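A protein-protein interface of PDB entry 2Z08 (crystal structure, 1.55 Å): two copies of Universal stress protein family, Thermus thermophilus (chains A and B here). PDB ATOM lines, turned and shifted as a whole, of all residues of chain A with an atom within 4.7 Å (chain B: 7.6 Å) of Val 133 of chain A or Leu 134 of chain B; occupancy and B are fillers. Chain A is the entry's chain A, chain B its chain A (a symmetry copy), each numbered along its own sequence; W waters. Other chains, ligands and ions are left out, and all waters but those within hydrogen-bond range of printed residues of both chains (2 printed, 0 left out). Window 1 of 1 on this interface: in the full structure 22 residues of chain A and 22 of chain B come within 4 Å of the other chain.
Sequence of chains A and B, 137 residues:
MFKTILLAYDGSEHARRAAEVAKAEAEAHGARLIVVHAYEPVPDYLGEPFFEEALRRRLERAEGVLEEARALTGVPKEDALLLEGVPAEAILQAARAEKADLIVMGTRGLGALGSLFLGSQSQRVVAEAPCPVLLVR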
ATOM      1  N   PHE A   2     -15.161 -18.404  -0.354  1.00  0.00           N
ATOM      2  CA  PHE A   2     -14.500 -19.109  -1.475  1.00  0.00           C
ATOM      3  C   PHE A   2     -12.964 -18.881  -1.339  1.00  0.00           C
ATOM      4  O   PHE A   2     -12.389 -17.853  -1.706  1.00  0.00           O
ATOM      5  CB  PHE A   2     -14.935 -18.591  -2.864  1.00  0.00           C
ATOM      6  CG  PHE A   2     -16.440 -18.782  -3.196  1.00  0.00           C
ATOM      7  CD1 PHE A   2     -17.074 -17.863  -4.031  1.00  0.00           C
ATOM      8  CD2 PHE A   2     -17.205 -19.837  -2.700  1.00  0.00           C
ATOM      9  CE1 PHE A   2     -18.398 -17.959  -4.334  1.00  0.00           C
ATOM     10  CE2 PHE A   2     -18.622 -19.974  -3.005  1.00  0.00           C
ATOM     11  CZ  PHE A   2     -19.230 -19.004  -3.837  1.00  0.00           C
ATOM     12  N   LEU A 102     -16.030 -23.744  -4.529  1.00  0.00           N
ATOM     13  CA  LEU A 102     -16.850 -23.364  -5.690  1.00  0.00           C
ATOM     14  C   LEU A 102     -16.301 -24.205  -6.846  1.00  0.00           C
ATOM     15  O   LEU A 102     -15.073 -24.377  -6.958  1.00  0.00           O
ATOM     16  CB  LEU A 102     -16.644 -21.871  -6.008  1.00  0.00           C
ATOM     17  CG  LEU A 102     -17.355 -21.325  -7.247  1.00  0.00           C
ATOM     18  CD1 LEU A 102     -18.873 -21.376  -7.014  1.00  0.00           C
ATOM     19  CD2 LEU A 102     -16.878 -19.929  -7.590  1.00  0.00           C
ATOM     20  N   ILE A 103     -17.177 -24.729  -7.679  1.00  0.00           N
ATOM     21  CA  ILE A 103     -16.849 -25.367  -8.930  1.00  0.00           C
ATOM     22  C   ILE A 103     -17.345 -24.442 -10.041  1.00  0.00           C
ATOM     23  O   ILE A 103     -18.503 -24.009  -9.906  1.00  0.00           O
ATOM     24  CB  ILE A 103     -17.527 -26.715  -9.124  1.00  0.00           C
ATOM     25  CG1 ILE A 103     -16.927 -27.663  -8.060  1.00  0.00           C
ATOM     26  CG2 ILE A 103     -17.314 -27.230 -10.461  1.00  0.00           C
ATOM     27  CD1 ILE A 103     -15.638 -27.766  -7.935  1.00  0.00           C
ATOM     28  N   MET A 105     -18.004 -24.237 -14.214  1.00  0.00           N
ATOM     29  CA  MET A 105     -17.881 -25.051 -15.407  1.00  0.00           C
ATOM     30  C   MET A 105     -18.911 -24.504 -16.453  1.00  0.00           C
ATOM     31  O   MET A 105     -19.747 -23.705 -16.046  1.00  0.00           O
ATOM     32  CB  MET A 105     -18.233 -26.545 -15.058  1.00  0.00           C
ATOM     33  CG  MET A 105     -19.692 -26.746 -14.656  1.00  0.00           C
ATOM     34  SD  MET A 105     -19.810 -28.385 -13.715  1.00  0.00           S
ATOM     35  CE  MET A 105     -19.241 -29.531 -15.024  1.00  0.00           C
ATOM     36  N   VAL A 125     -22.481 -33.080 -12.020  1.00  0.00           N
ATOM     37  CA  VAL A 125     -21.823 -32.360 -10.934  1.00  0.00           C
ATOM     38  C   VAL A 125     -22.777 -31.585 -10.052  1.00  0.00           C
ATOM     39  O   VAL A 125     -22.637 -31.611  -8.849  1.00  0.00           O
ATOM     40  CB  VAL A 125     -20.746 -31.392 -11.565  1.00  0.00           C
ATOM     41  CG1 VAL A 125     -20.116 -30.521 -10.457  1.00  0.00           C
ATOM     42  CG2 VAL A 125     -19.654 -32.167 -12.208  1.00  0.00           C
ATOM     43  N   VAL A 126     -23.758 -30.945 -10.655  1.00  0.00           N
ATOM     44  CA  VAL A 126     -24.741 -30.185  -9.875  1.00  0.00           C
ATOM     45  C   VAL A 126     -25.483 -31.161  -8.978  1.00  0.00           C
ATOM     46  O   VAL A 126     -25.801 -30.758  -7.860  1.00  0.00           O
ATOM     47  CB  VAL A 126     -25.732 -29.469 -10.792  1.00  0.00           C
ATOM     48  CG1 VAL A 126     -26.944 -28.932  -9.984  1.00  0.00           C
ATOM     49  CG2 VAL A 126     -25.025 -28.315 -11.546  1.00  0.00           C
ATOM     50  N   ALA A 129     -22.712 -32.186  -6.181  1.00  0.00           N
ATOM     51  CA  ALA A 129     -21.637 -31.276  -5.750  1.00  0.00           C
ATOM     52  C   ALA A 129     -21.445 -31.034  -4.239  1.00  0.00           C
ATOM     53  O   ALA A 129     -22.409 -30.991  -3.535  1.00  0.00           O
ATOM     54  CB  ALA A 129     -21.772 -29.929  -6.411  1.00  0.00           C
ATOM     55  N   CYS A 131     -20.346 -28.367  -3.074  1.00  0.00           N
ATOM     56  CA  CYS A 131     -20.244 -26.919  -2.839  1.00  0.00           C
ATOM     57  C   CYS A 131     -21.052 -26.243  -3.986  1.00  0.00           C
ATOM     58  O   CYS A 131     -21.495 -26.962  -4.879  1.00  0.00           O
ATOM     59  CB  CYS A 131     -18.778 -26.464  -2.977  1.00  0.00           C
ATOM     60  SG  CYS A 131     -18.003 -26.961  -4.574  1.00  0.00           S
ATOM     61  N   PRO A 132     -21.188 -24.938  -3.973  1.00  0.00           N
ATOM     62  CA  PRO A 132     -21.902 -24.288  -5.048  1.00  0.00           C
ATOM     63  C   PRO A 132     -21.220 -24.505  -6.398  1.00  0.00           C
ATOM     64  O   PRO A 132     -19.994 -24.760  -6.514  1.00  0.00           O
ATOM     65  CB  PRO A 132     -21.893 -22.848  -4.659  1.00  0.00           C
ATOM     66  CG  PRO A 132     -21.869 -22.812  -3.104  1.00  0.00           C
ATOM     67  CD  PRO A 132     -20.883 -24.011  -2.844  1.00  0.00           C
ATOM     68  N   VAL A 133     -22.062 -24.390  -7.460  1.00  0.00           N
ATOM     69  CA  VAL A 133     -21.546 -24.609  -8.811  1.00  0.00           C
ATOM     70  C   VAL A 133     -21.976 -23.358  -9.619  1.00  0.00           C
ATOM     71  O   VAL A 133     -23.143 -22.998  -9.619  1.00  0.00           O
ATOM     72  CB  VAL A 133     -22.263 -25.833  -9.444  1.00  0.00           C
ATOM     73  CG1 VAL A 133     -21.745 -26.005 -10.912  1.00  0.00           C
ATOM     74  CG2 VAL A 133     -21.868 -27.065  -8.612  1.00  0.00           C
ATOM     75  N   LEU A 134     -21.003 -22.730 -10.258  1.00  0.00           N
ATOM     76  CA  LEU A 134     -21.214 -21.539 -11.112  1.00  0.00           C
ATOM     77  C   LEU A 134     -21.186 -22.033 -12.546  1.00  0.00           C
ATOM     78  O   LEU A 134     -20.141 -22.461 -13.064  1.00  0.00           O
ATOM     79  CB  LEU A 134     -20.067 -20.518 -10.843  1.00  0.00           C
ATOM     80  CG  LEU A 134     -20.105 -19.245 -11.634  1.00  0.00           C
ATOM     81  CD1 LEU A 134     -21.343 -18.692 -11.669  1.00  0.00           C
ATOM     82  CD2 LEU A 134     -19.207 -18.243 -10.929  1.00  0.00           C
ATOM     83  N   LEU A 135     -22.343 -21.991 -13.203  1.00  0.00           N
ATOM     84  CA  LEU A 135     -22.587 -22.459 -14.595  1.00  0.00           C
ATOM     85  C   LEU A 135     -22.425 -21.292 -15.528  1.00  0.00           C
ATOM     86  O   LEU A 135     -23.115 -20.280 -15.352  1.00  0.00           O
ATOM     87  CB  LEU A 135     -23.986 -23.057 -14.739  1.00  0.00           C
ATOM     88  CG  LEU A 135     -24.191 -24.420 -13.940  1.00  0.00           C
ATOM     89  CD1 LEU A 135     -25.616 -24.798 -14.055  1.00  0.00           C
ATOM     90  CD2 LEU A 135     -23.261 -25.512 -14.492  1.00  0.00           C
ATOM     91  N   PHE B   2     -18.872  -8.879 -13.120  1.00  0.00           N
ATOM     92  CA  PHE B   2     -20.147  -8.908 -12.369  1.00  0.00           C
ATOM     93  C   PHE B   2     -20.331  -7.518 -11.690  1.00  0.00           C
ATOM     94  O   PHE B   2     -19.772  -7.189 -10.640  1.00  0.00           O
ATOM     95  CB  PHE B   2     -20.178  -9.985 -11.261  1.00  0.00           C
ATOM     96  CG  PHE B   2     -20.057 -11.450 -11.762  1.00  0.00           C
ATOM     97  CD1 PHE B   2     -19.449 -12.400 -10.943  1.00  0.00           C
ATOM     98  CD2 PHE B   2     -20.528 -11.876 -13.003  1.00  0.00           C
ATOM     99  CE1 PHE B   2     -19.285 -13.693 -11.339  1.00  0.00           C
ATOM    100  CE2 PHE B   2     -20.373 -13.249 -13.459  1.00  0.00           C
ATOM    101  CZ  PHE B   2     -19.729 -14.175 -12.604  1.00  0.00           C
ATOM    102  N   ILE B   5     -25.763  -8.255  -9.720  1.00  0.00           N
ATOM    103  CA  ILE B   5     -26.062  -9.625  -9.325  1.00  0.00           C
ATOM    104  C   ILE B   5     -27.488  -9.694  -8.952  1.00  0.00           C
ATOM    105  O   ILE B   5     -27.971  -8.817  -8.269  1.00  0.00           O
ATOM    106  CB  ILE B   5     -25.189 -10.031  -8.134  1.00  0.00           C
ATOM    107  CG1 ILE B   5     -23.675  -9.859  -8.443  1.00  0.00           C
ATOM    108  CG2 ILE B   5     -25.522 -11.473  -7.720  1.00  0.00           C
ATOM    109  CD1 ILE B   5     -22.796 -10.056  -7.331  1.00  0.00           C
ATOM    110  N   LEU B   6     -28.182 -10.758  -9.367  1.00  0.00           N
ATOM    111  CA  LEU B   6     -29.590 -10.939  -8.968  1.00  0.00           C
ATOM    112  C   LEU B   6     -29.710 -12.216  -8.142  1.00  0.00           C
ATOM    113  O   LEU B   6     -29.289 -13.257  -8.650  1.00  0.00           O
ATOM    114  CB  LEU B   6     -30.476 -10.994 -10.262  1.00  0.00           C
ATOM    115  CG  LEU B   6     -31.968 -11.032  -9.937  1.00  0.00           C
ATOM    116  CD1 LEU B   6     -32.830 -10.347 -10.920  1.00  0.00           C
ATOM    117  CD2 LEU B   6     -32.395 -12.352  -9.850  1.00  0.00           C
ATOM    118  N   LEU B   7     -30.300 -12.113  -6.957  1.00  0.00           N
ATOM    119  CA  LEU B   7     -30.597 -13.226  -6.066  1.00  0.00           C
ATOM    120  C   LEU B   7     -32.080 -13.605  -6.210  1.00  0.00           C
ATOM    121  O   LEU B   7     -32.923 -12.719  -6.013  1.00  0.00           O
ATOM    122  CB  LEU B   7     -30.367 -12.820  -4.610  1.00  0.00           C
ATOM    123  CG  LEU B   7     -30.948 -13.869  -3.612  1.00  0.00           C
ATOM    124  CD1 LEU B   7     -30.173 -15.201  -3.656  1.00  0.00           C
ATOM    125  CD2 LEU B   7     -30.802 -13.173  -2.213  1.00  0.00           C
ATOM    126  N   ALA B  18     -28.102 -19.203  -0.397  1.00  0.00           N
ATOM    127  CA  ALA B  18     -27.837 -18.425  -1.564  1.00  0.00           C
ATOM    128  C   ALA B  18     -27.728 -16.925  -1.278  1.00  0.00           C
ATOM    129  O   ALA B  18     -27.005 -16.196  -1.998  1.00  0.00           O
ATOM    130  CB  ALA B  18     -29.026 -18.746  -2.616  1.00  0.00           C
ATOM    131  N   VAL B  21     -24.323 -16.230  -0.046  1.00  0.00           N
ATOM    132  CA  VAL B  21     -23.371 -16.267  -1.160  1.00  0.00           C
ATOM    133  C   VAL B  21     -23.517 -15.027  -2.022  1.00  0.00           C
ATOM    134  O   VAL B  21     -22.502 -14.449  -2.474  1.00  0.00           O
ATOM    135  CB  VAL B  21     -23.564 -17.547  -2.071  1.00  0.00           C
ATOM    136  CG1 VAL B  21     -22.766 -17.437  -3.414  1.00  0.00           C
ATOM    137  CG2 VAL B  21     -23.129 -18.803  -1.308  1.00  0.00           C
ATOM    138  N   ALA B  22     -24.751 -14.606  -2.286  1.00  0.00           N
ATOM    139  CA  ALA B  22     -24.978 -13.433  -3.131  1.00  0.00           C
ATOM    140  C   ALA B  22     -24.399 -12.171  -2.475  1.00  0.00           C
ATOM    141  O   ALA B  22     -23.841 -11.400  -3.146  1.00  0.00           O
ATOM    142  CB  ALA B  22     -26.526 -13.190  -3.428  1.00  0.00           C
ATOM    143  N   GLU B  25     -20.585 -12.235  -2.848  1.00  0.00           N
ATOM    144  CA  GLU B  25     -20.218 -12.021  -4.232  1.00  0.00           C
ATOM    145  C   GLU B  25     -20.354 -10.542  -4.542  1.00  0.00           C
ATOM    146  O   GLU B  25     -19.531 -10.008  -5.189  1.00  0.00           O
ATOM    147  CB  GLU B  25     -21.154 -12.785  -5.208  1.00  0.00           C
ATOM    148  CG  GLU B  25     -20.871 -14.246  -5.377  1.00  0.00           C
ATOM    149  CD  GLU B  25     -19.560 -14.550  -6.171  1.00  0.00           C
ATOM    150  OE1 GLU B  25     -19.522 -15.494  -6.990  1.00  0.00           O
ATOM    151  OE2 GLU B  25     -18.570 -13.898  -5.951  1.00  0.00           O
ATOM    152  N   LEU B 102     -24.997 -11.910 -13.158  1.00  0.00           N
ATOM    153  CA  LEU B 102     -24.938 -13.202 -12.456  1.00  0.00           C
ATOM    154  C   LEU B 102     -26.313 -13.349 -11.797  1.00  0.00           C
ATOM    155  O   LEU B 102     -26.858 -12.359 -11.274  1.00  0.00           O
ATOM    156  CB  LEU B 102     -23.856 -13.151 -11.362  1.00  0.00           C
ATOM    157  CG  LEU B 102     -23.720 -14.386 -10.469  1.00  0.00           C
ATOM    158  CD1 LEU B 102     -23.231 -15.567 -11.322  1.00  0.00           C
ATOM    159  CD2 LEU B 102     -22.808 -14.120  -9.290  1.00  0.00           C
ATOM    160  N   ILE B 103     -26.871 -14.542 -11.829  1.00  0.00           N
ATOM    161  CA  ILE B 103     -28.050 -14.923 -11.090  1.00  0.00           C
ATOM    162  C   ILE B 103     -27.595 -15.897 -10.004  1.00  0.00           C
ATOM    163  O   ILE B 103     -26.837 -16.808 -10.380  1.00  0.00           O
ATOM    164  CB  ILE B 103     -29.095 -15.637 -11.934  1.00  0.00           C
ATOM    165  CG1 ILE B 103     -29.619 -14.598 -12.952  1.00  0.00           C
ATOM    166  CG2 ILE B 103     -30.173 -16.157 -11.118  1.00  0.00           C
ATOM    167  CD1 ILE B 103     -30.021 -13.432 -12.542  1.00  0.00           C
ATOM    168  N   VAL B 104     -27.991 -15.689  -8.732  1.00  0.00           N
ATOM    169  CA  VAL B 104     -27.624 -16.632  -7.686  1.00  0.00           C
ATOM    170  C   VAL B 104     -28.925 -17.261  -7.193  1.00  0.00           C
ATOM    171  O   VAL B 104     -29.897 -16.520  -6.965  1.00  0.00           O
ATOM    172  CB  VAL B 104     -26.953 -15.882  -6.514  1.00  0.00           C
ATOM    173  CG1 VAL B 104     -26.461 -16.891  -5.385  1.00  0.00           C
ATOM    174  CG2 VAL B 104     -25.689 -15.108  -7.115  1.00  0.00           C
ATOM    175  N   MET B 105     -29.031 -18.609  -7.093  1.00  0.00           N
ATOM    176  CA  MET B 105     -30.277 -19.139  -6.576  1.00  0.00           C
ATOM    177  C   MET B 105     -29.966 -20.547  -5.964  1.00  0.00           C
ATOM    178  O   MET B 105     -28.868 -21.033  -6.213  1.00  0.00           O
ATOM    179  CB  MET B 105     -31.305 -19.298  -7.758  1.00  0.00           C
ATOM    180  CG  MET B 105     -30.890 -20.345  -8.788  1.00  0.00           C
ATOM    181  SD  MET B 105     -31.854 -20.002 -10.381  1.00  0.00           S
ATOM    182  CE  MET B 105     -33.562 -20.218  -9.757  1.00  0.00           C
ATOM    183  N   GLY B 106     -30.865 -21.123  -5.191  1.00  0.00           N
ATOM    184  CA  GLY B 106     -30.573 -22.436  -4.664  1.00  0.00           C
ATOM    185  C   GLY B 106     -30.730 -23.509  -5.700  1.00  0.00           C
ATOM    186  O   GLY B 106     -31.387 -23.334  -6.734  1.00  0.00           O
ATOM    187  N   THR B 107     -30.108 -24.668  -5.395  1.00  0.00           N
ATOM    188  CA  THR B 107     -30.373 -25.795  -6.297  1.00  0.00           C
ATOM    189  C   THR B 107     -31.823 -26.303  -6.152  1.00  0.00           C
ATOM    190  O   THR B 107     -32.373 -26.823  -7.116  1.00  0.00           O
ATOM    191  CB  THR B 107     -29.376 -26.951  -5.982  1.00  0.00           C
ATOM    192  OG1 THR B 107     -29.493 -27.184  -4.537  1.00  0.00           O
ATOM    193  CG2 THR B 107     -27.954 -26.628  -6.377  1.00  0.00           C
ATOM    194  N   SER B 122     -34.969 -23.585 -10.932  1.00  0.00           N
ATOM    195  CA  SER B 122     -33.584 -23.493 -11.326  1.00  0.00           C
ATOM    196  C   SER B 122     -33.301 -24.138 -12.714  1.00  0.00           C
ATOM    197  O   SER B 122     -32.507 -23.541 -13.458  1.00  0.00           O
ATOM    198  CB  SER B 122     -32.693 -24.189 -10.341  1.00  0.00           C
ATOM    199  OG  SER B 122     -32.686 -23.440  -9.124  1.00  0.00           O
ATOM    200  N   VAL B 126     -31.603 -21.868 -15.668  1.00  0.00           N
ATOM    201  CA  VAL B 126     -30.336 -22.288 -16.277  1.00  0.00           C
ATOM    202  C   VAL B 126     -30.575 -22.485 -17.764  1.00  0.00           C
ATOM    203  O   VAL B 126     -29.658 -22.170 -18.522  1.00  0.00           O
ATOM    204  CB  VAL B 126     -29.837 -23.591 -15.656  1.00  0.00           C
ATOM    205  CG1 VAL B 126     -28.684 -24.200 -16.499  1.00  0.00           C
ATOM    206  CG2 VAL B 126     -29.374 -23.347 -14.198  1.00  0.00           C
ATOM    207  N   CYS B 131     -27.100 -14.971 -18.481  1.00  0.00           N
ATOM    208  CA  CYS B 131     -25.788 -14.726 -17.863  1.00  0.00           C
ATOM    209  C   CYS B 131     -25.473 -15.993 -17.014  1.00  0.00           C
ATOM    210  O   CYS B 131     -26.348 -16.851 -16.914  1.00  0.00           O
ATOM    211  CB  CYS B 131     -25.875 -13.531 -16.895  1.00  0.00           C
ATOM    212  SG  CYS B 131     -27.209 -13.703 -15.635  1.00  0.00           S
ATOM    213  N   PRO B 132     -24.311 -16.070 -16.409  1.00  0.00           N
ATOM    214  CA  PRO B 132     -24.015 -17.219 -15.585  1.00  0.00           C
ATOM    215  C   PRO B 132     -24.976 -17.337 -14.404  1.00  0.00           C
ATOM    216  O   PRO B 132     -25.594 -16.354 -13.921  1.00  0.00           O
ATOM    217  CB  PRO B 132     -22.617 -16.975 -15.127  1.00  0.00           C
ATOM    218  CG  PRO B 132     -21.923 -16.152 -16.249  1.00  0.00           C
ATOM    219  CD  PRO B 132     -23.118 -15.203 -16.635  1.00  0.00           C
ATOM    220  N   VAL B 133     -25.097 -18.603 -13.921  1.00  0.00           N
ATOM    221  CA  VAL B 133     -26.013 -18.864 -12.811  1.00  0.00           C
ATOM    222  C   VAL B 133     -25.167 -19.618 -11.754  1.00  0.00           C
ATOM    223  O   VAL B 133     -24.527 -20.608 -12.070  1.00  0.00           O
ATOM    224  CB  VAL B 133     -27.129 -19.835 -13.283  1.00  0.00           C
ATOM    225  CG1 VAL B 133     -28.057 -20.153 -12.062  1.00  0.00           C
ATOM    226  CG2 VAL B 133     -27.939 -19.098 -14.365  1.00  0.00           C
ATOM    227  N   LEU B 134     -25.182 -19.098 -10.537  1.00  0.00           N
ATOM    228  CA  LEU B 134     -24.470 -19.690  -9.381  1.00  0.00           C
ATOM    229  C   LEU B 134     -25.519 -20.418  -8.562  1.00  0.00           C
ATOM    230  O   LEU B 134     -26.406 -19.801  -7.949  1.00  0.00           O
ATOM    231  CB  LEU B 134     -23.807 -18.543  -8.560  1.00  0.00           C
ATOM    232  CG  LEU B 134     -23.046 -18.952  -7.333  1.00  0.00           C
ATOM    233  CD1 LEU B 134     -22.236 -20.017  -7.556  1.00  0.00           C
ATOM    234  CD2 LEU B 134     -22.140 -17.795  -6.951  1.00  0.00           C
ATOM    235  N   LEU B 135     -25.438 -21.747  -8.552  1.00  0.00           N
ATOM    236  CA  LEU B 135     -26.369 -22.686  -7.869  1.00  0.00           C
ATOM    237  C   LEU B 135     -25.817 -22.998  -6.506  1.00  0.00           C
ATOM    238  O   LEU B 135     -24.678 -23.474  -6.412  1.00  0.00           O
ATOM    239  CB  LEU B 135     -26.545 -23.972  -8.673  1.00  0.00           C
ATOM    240  CG  LEU B 135     -27.309 -23.770 -10.057  1.00  0.00           C
ATOM    241  CD1 LEU B 135     -27.276 -25.059 -10.780  1.00  0.00           C
ATOM    242  CD2 LEU B 135     -28.746 -23.286  -9.810  1.00  0.00           C
ATOM    243  N   VAL B 136     -26.592 -22.712  -5.470  1.00  0.00           N
ATOM    244  CA  VAL B 136     -26.139 -22.923  -4.051  1.00  0.00           C
ATOM    245  C   VAL B 136     -26.926 -24.032  -3.438  1.00  0.00           C
ATOM    246  O   VAL B 136     -28.098 -23.998  -3.413  1.00  0.00           O
ATOM    247  CB  VAL B 136     -26.365 -21.607  -3.315  1.00  0.00           C
ATOM    248  CG1 VAL B 136     -25.910 -21.776  -1.838  1.00  0.00           C
ATOM    249  CG2 VAL B 136     -25.516 -20.494  -3.925  1.00  0.00           C
ATOM    250  N   ARG B 137     -26.235 -25.104  -2.981  1.00  0.00           N
ATOM    251  CA  ARG B 137     -26.888 -26.238  -2.348  1.00  0.00           C
ATOM    252  C   ARG B 137     -27.094 -26.028  -0.858  1.00  0.00           C
ATOM    253  O   ARG B 137     -26.625 -25.053  -0.287  1.00  0.00           O
ATOM    254  CB  ARG B 137     -26.070 -27.517  -2.534  1.00  0.00           C
ATOM    255  CG  ARG B 137     -24.760 -27.357  -1.875  1.00  0.00           C
ATOM    256  CD  ARG B 137     -23.618 -28.398  -1.878  1.00  0.00           C
ATOM    257  NE  ARG B 137     -22.628 -27.505  -1.250  1.00  0.00           N
ATOM    258  CZ  ARG B 137     -22.569 -27.141   0.036  1.00  0.00           C
ATOM    259  NH1 ARG B 137     -23.388 -27.631   1.011  1.00  0.00           N
ATOM    260  NH2 ARG B 137     -21.896 -26.085   0.310  1.00  0.00           N
ATOM    261  OXT ARG B 137     -27.731 -26.923  -0.319  1.00  0.00           O
HETATM  262  O   HOH W   1     -24.469 -26.685  -5.721  1.00  0.00           O
HETATM  263  O   HOH W   2     -25.627 -19.825 -17.430  1.00  0.00           O
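The backbone carbonyl oxygen (O) of Val 133 of chain A sits at hydrogen-bond distance from the backbone NH (N) of Leu 135 of chain B (2.8 Å). O of Val 133 of chain B is in hydrogen-bond range of N of Leu 135 of chain A, at 2.8 Å. The backbone NH (N) of Cys 131 of chain A lies close to the guanidinium group (NE) of Arg 137 of chain B, at 3.0 Å.
The backbone NH (N) of Ile 103 of chain A lies within hydrogen-bond range of the backbone carbonyl oxygen (O) of Pro 132 of chain A, 3.0 Å away. O of Ile 103 of chain A sits at hydrogen-bond distance from N of Leu 134 of chain A (2.8 Å). The backbone NH (N) of Leu 6 of chain B sits at hydrogen-bond distance from the backbone carbonyl oxygen (O) of Leu 102 of chain B. The backbone NH (N) of Leu 102 of chain B is in hydrogen-bond range of the side-chain sulfur (SG) of Cys 131 of chain B. The backbone NH (N) of Ile 103 of chain B sits at hydrogen-bond distance from the backbone carbonyl oxygen (O) of Pro 132 of chain B, at 3.0 Å. O of Ile 103 of chain B lies within hydrogen-bond range of N of Leu 134 of chain B, at 2.8 Å.
Among the printed residues, pairs that only touch across the chains: Pro 132 of chain A with Leu 135 of chain B, Leu 135 of chain A with Pro 132 of chain B, Ala 129 of chain A with Arg 137 of chain B, Val 133 of chain A with Leu 134 of chain B, Leu 134 of chain A with Val 133 of chain B, Leu 102 of chain A with Leu 134 of chain B, Leu 134 of chain A with Leu 102 of chain B, Leu 135 of chain A with Leu 135 of chain B, Val 133 of chain A with Val 133 of chain B, Phe 2 of chain A with Glu 25 of chain B, Phe 2 of chain A with Val 21 of chain B, Pro 132 of chain A with Arg 137 of chain B, Leu 135 of chain A with Val 126 of chain B, Val 126 of chain A with Leu 135 of chain B and Leu 134 of chain A with Leu 134 of chain B.
Val 133 of chain A touches three residues of chain B. Of the printed residues of chain A, Glu 25 of chain B touches Phe 2. Of the printed residues of chain A, Leu 102 of chain B touches Leu 134. Cys 131 of chain B touches none of the printed residues of chain A. Of the printed residues of chain A, Leu 134 of chain B touches Leu 102, Val 133 and Leu 134. The nearest residue of chain A that does not touch Leu 134 of chain B is Pro 132 of chain A (4.1 Å). The nearest printed residue of chain B that does not touch Leu 102 of chain A is Glu 25 of chain B (5.2 Å).
Along chain B the printed residues that touch a printed residue of chain A span positions 21 to 137. Of the 12 printed residues of chain A, 9 touch a printed residue of chain B. Hydrophobic or aromatic side chains of chain A within 4 Å of the printed part of chain B: Phe 2, Leu 102, Val 126, Pro 132, Leu 134 and Leu 135.
Leu 102 of chain A touches Leu 134 of chain B, and with the chains exchanged Leu 134 of chain A touches Leu 102 of chain B. Val 126 of chain A touches Leu 135 of chain B, and with the chains exchanged Leu 135 of chain A touches Val 126 of chain B. Val 133 of chain A touches its own counterpart, Val 133 of chain B. Leu 134 of chain A touches its own counterpart, Leu 134 of chain B. Of the 18 pairs that touch across the chains among the printed residues, 13 have their exchanged pair printed and touching as well.
Water W2 lies within hydrogen-bond range of O of Cys 131 of chain B and O of Leu 135 of chain A. Water W1 bridges O of Cys 131 of chain A and O of Leu 135 of chain B.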
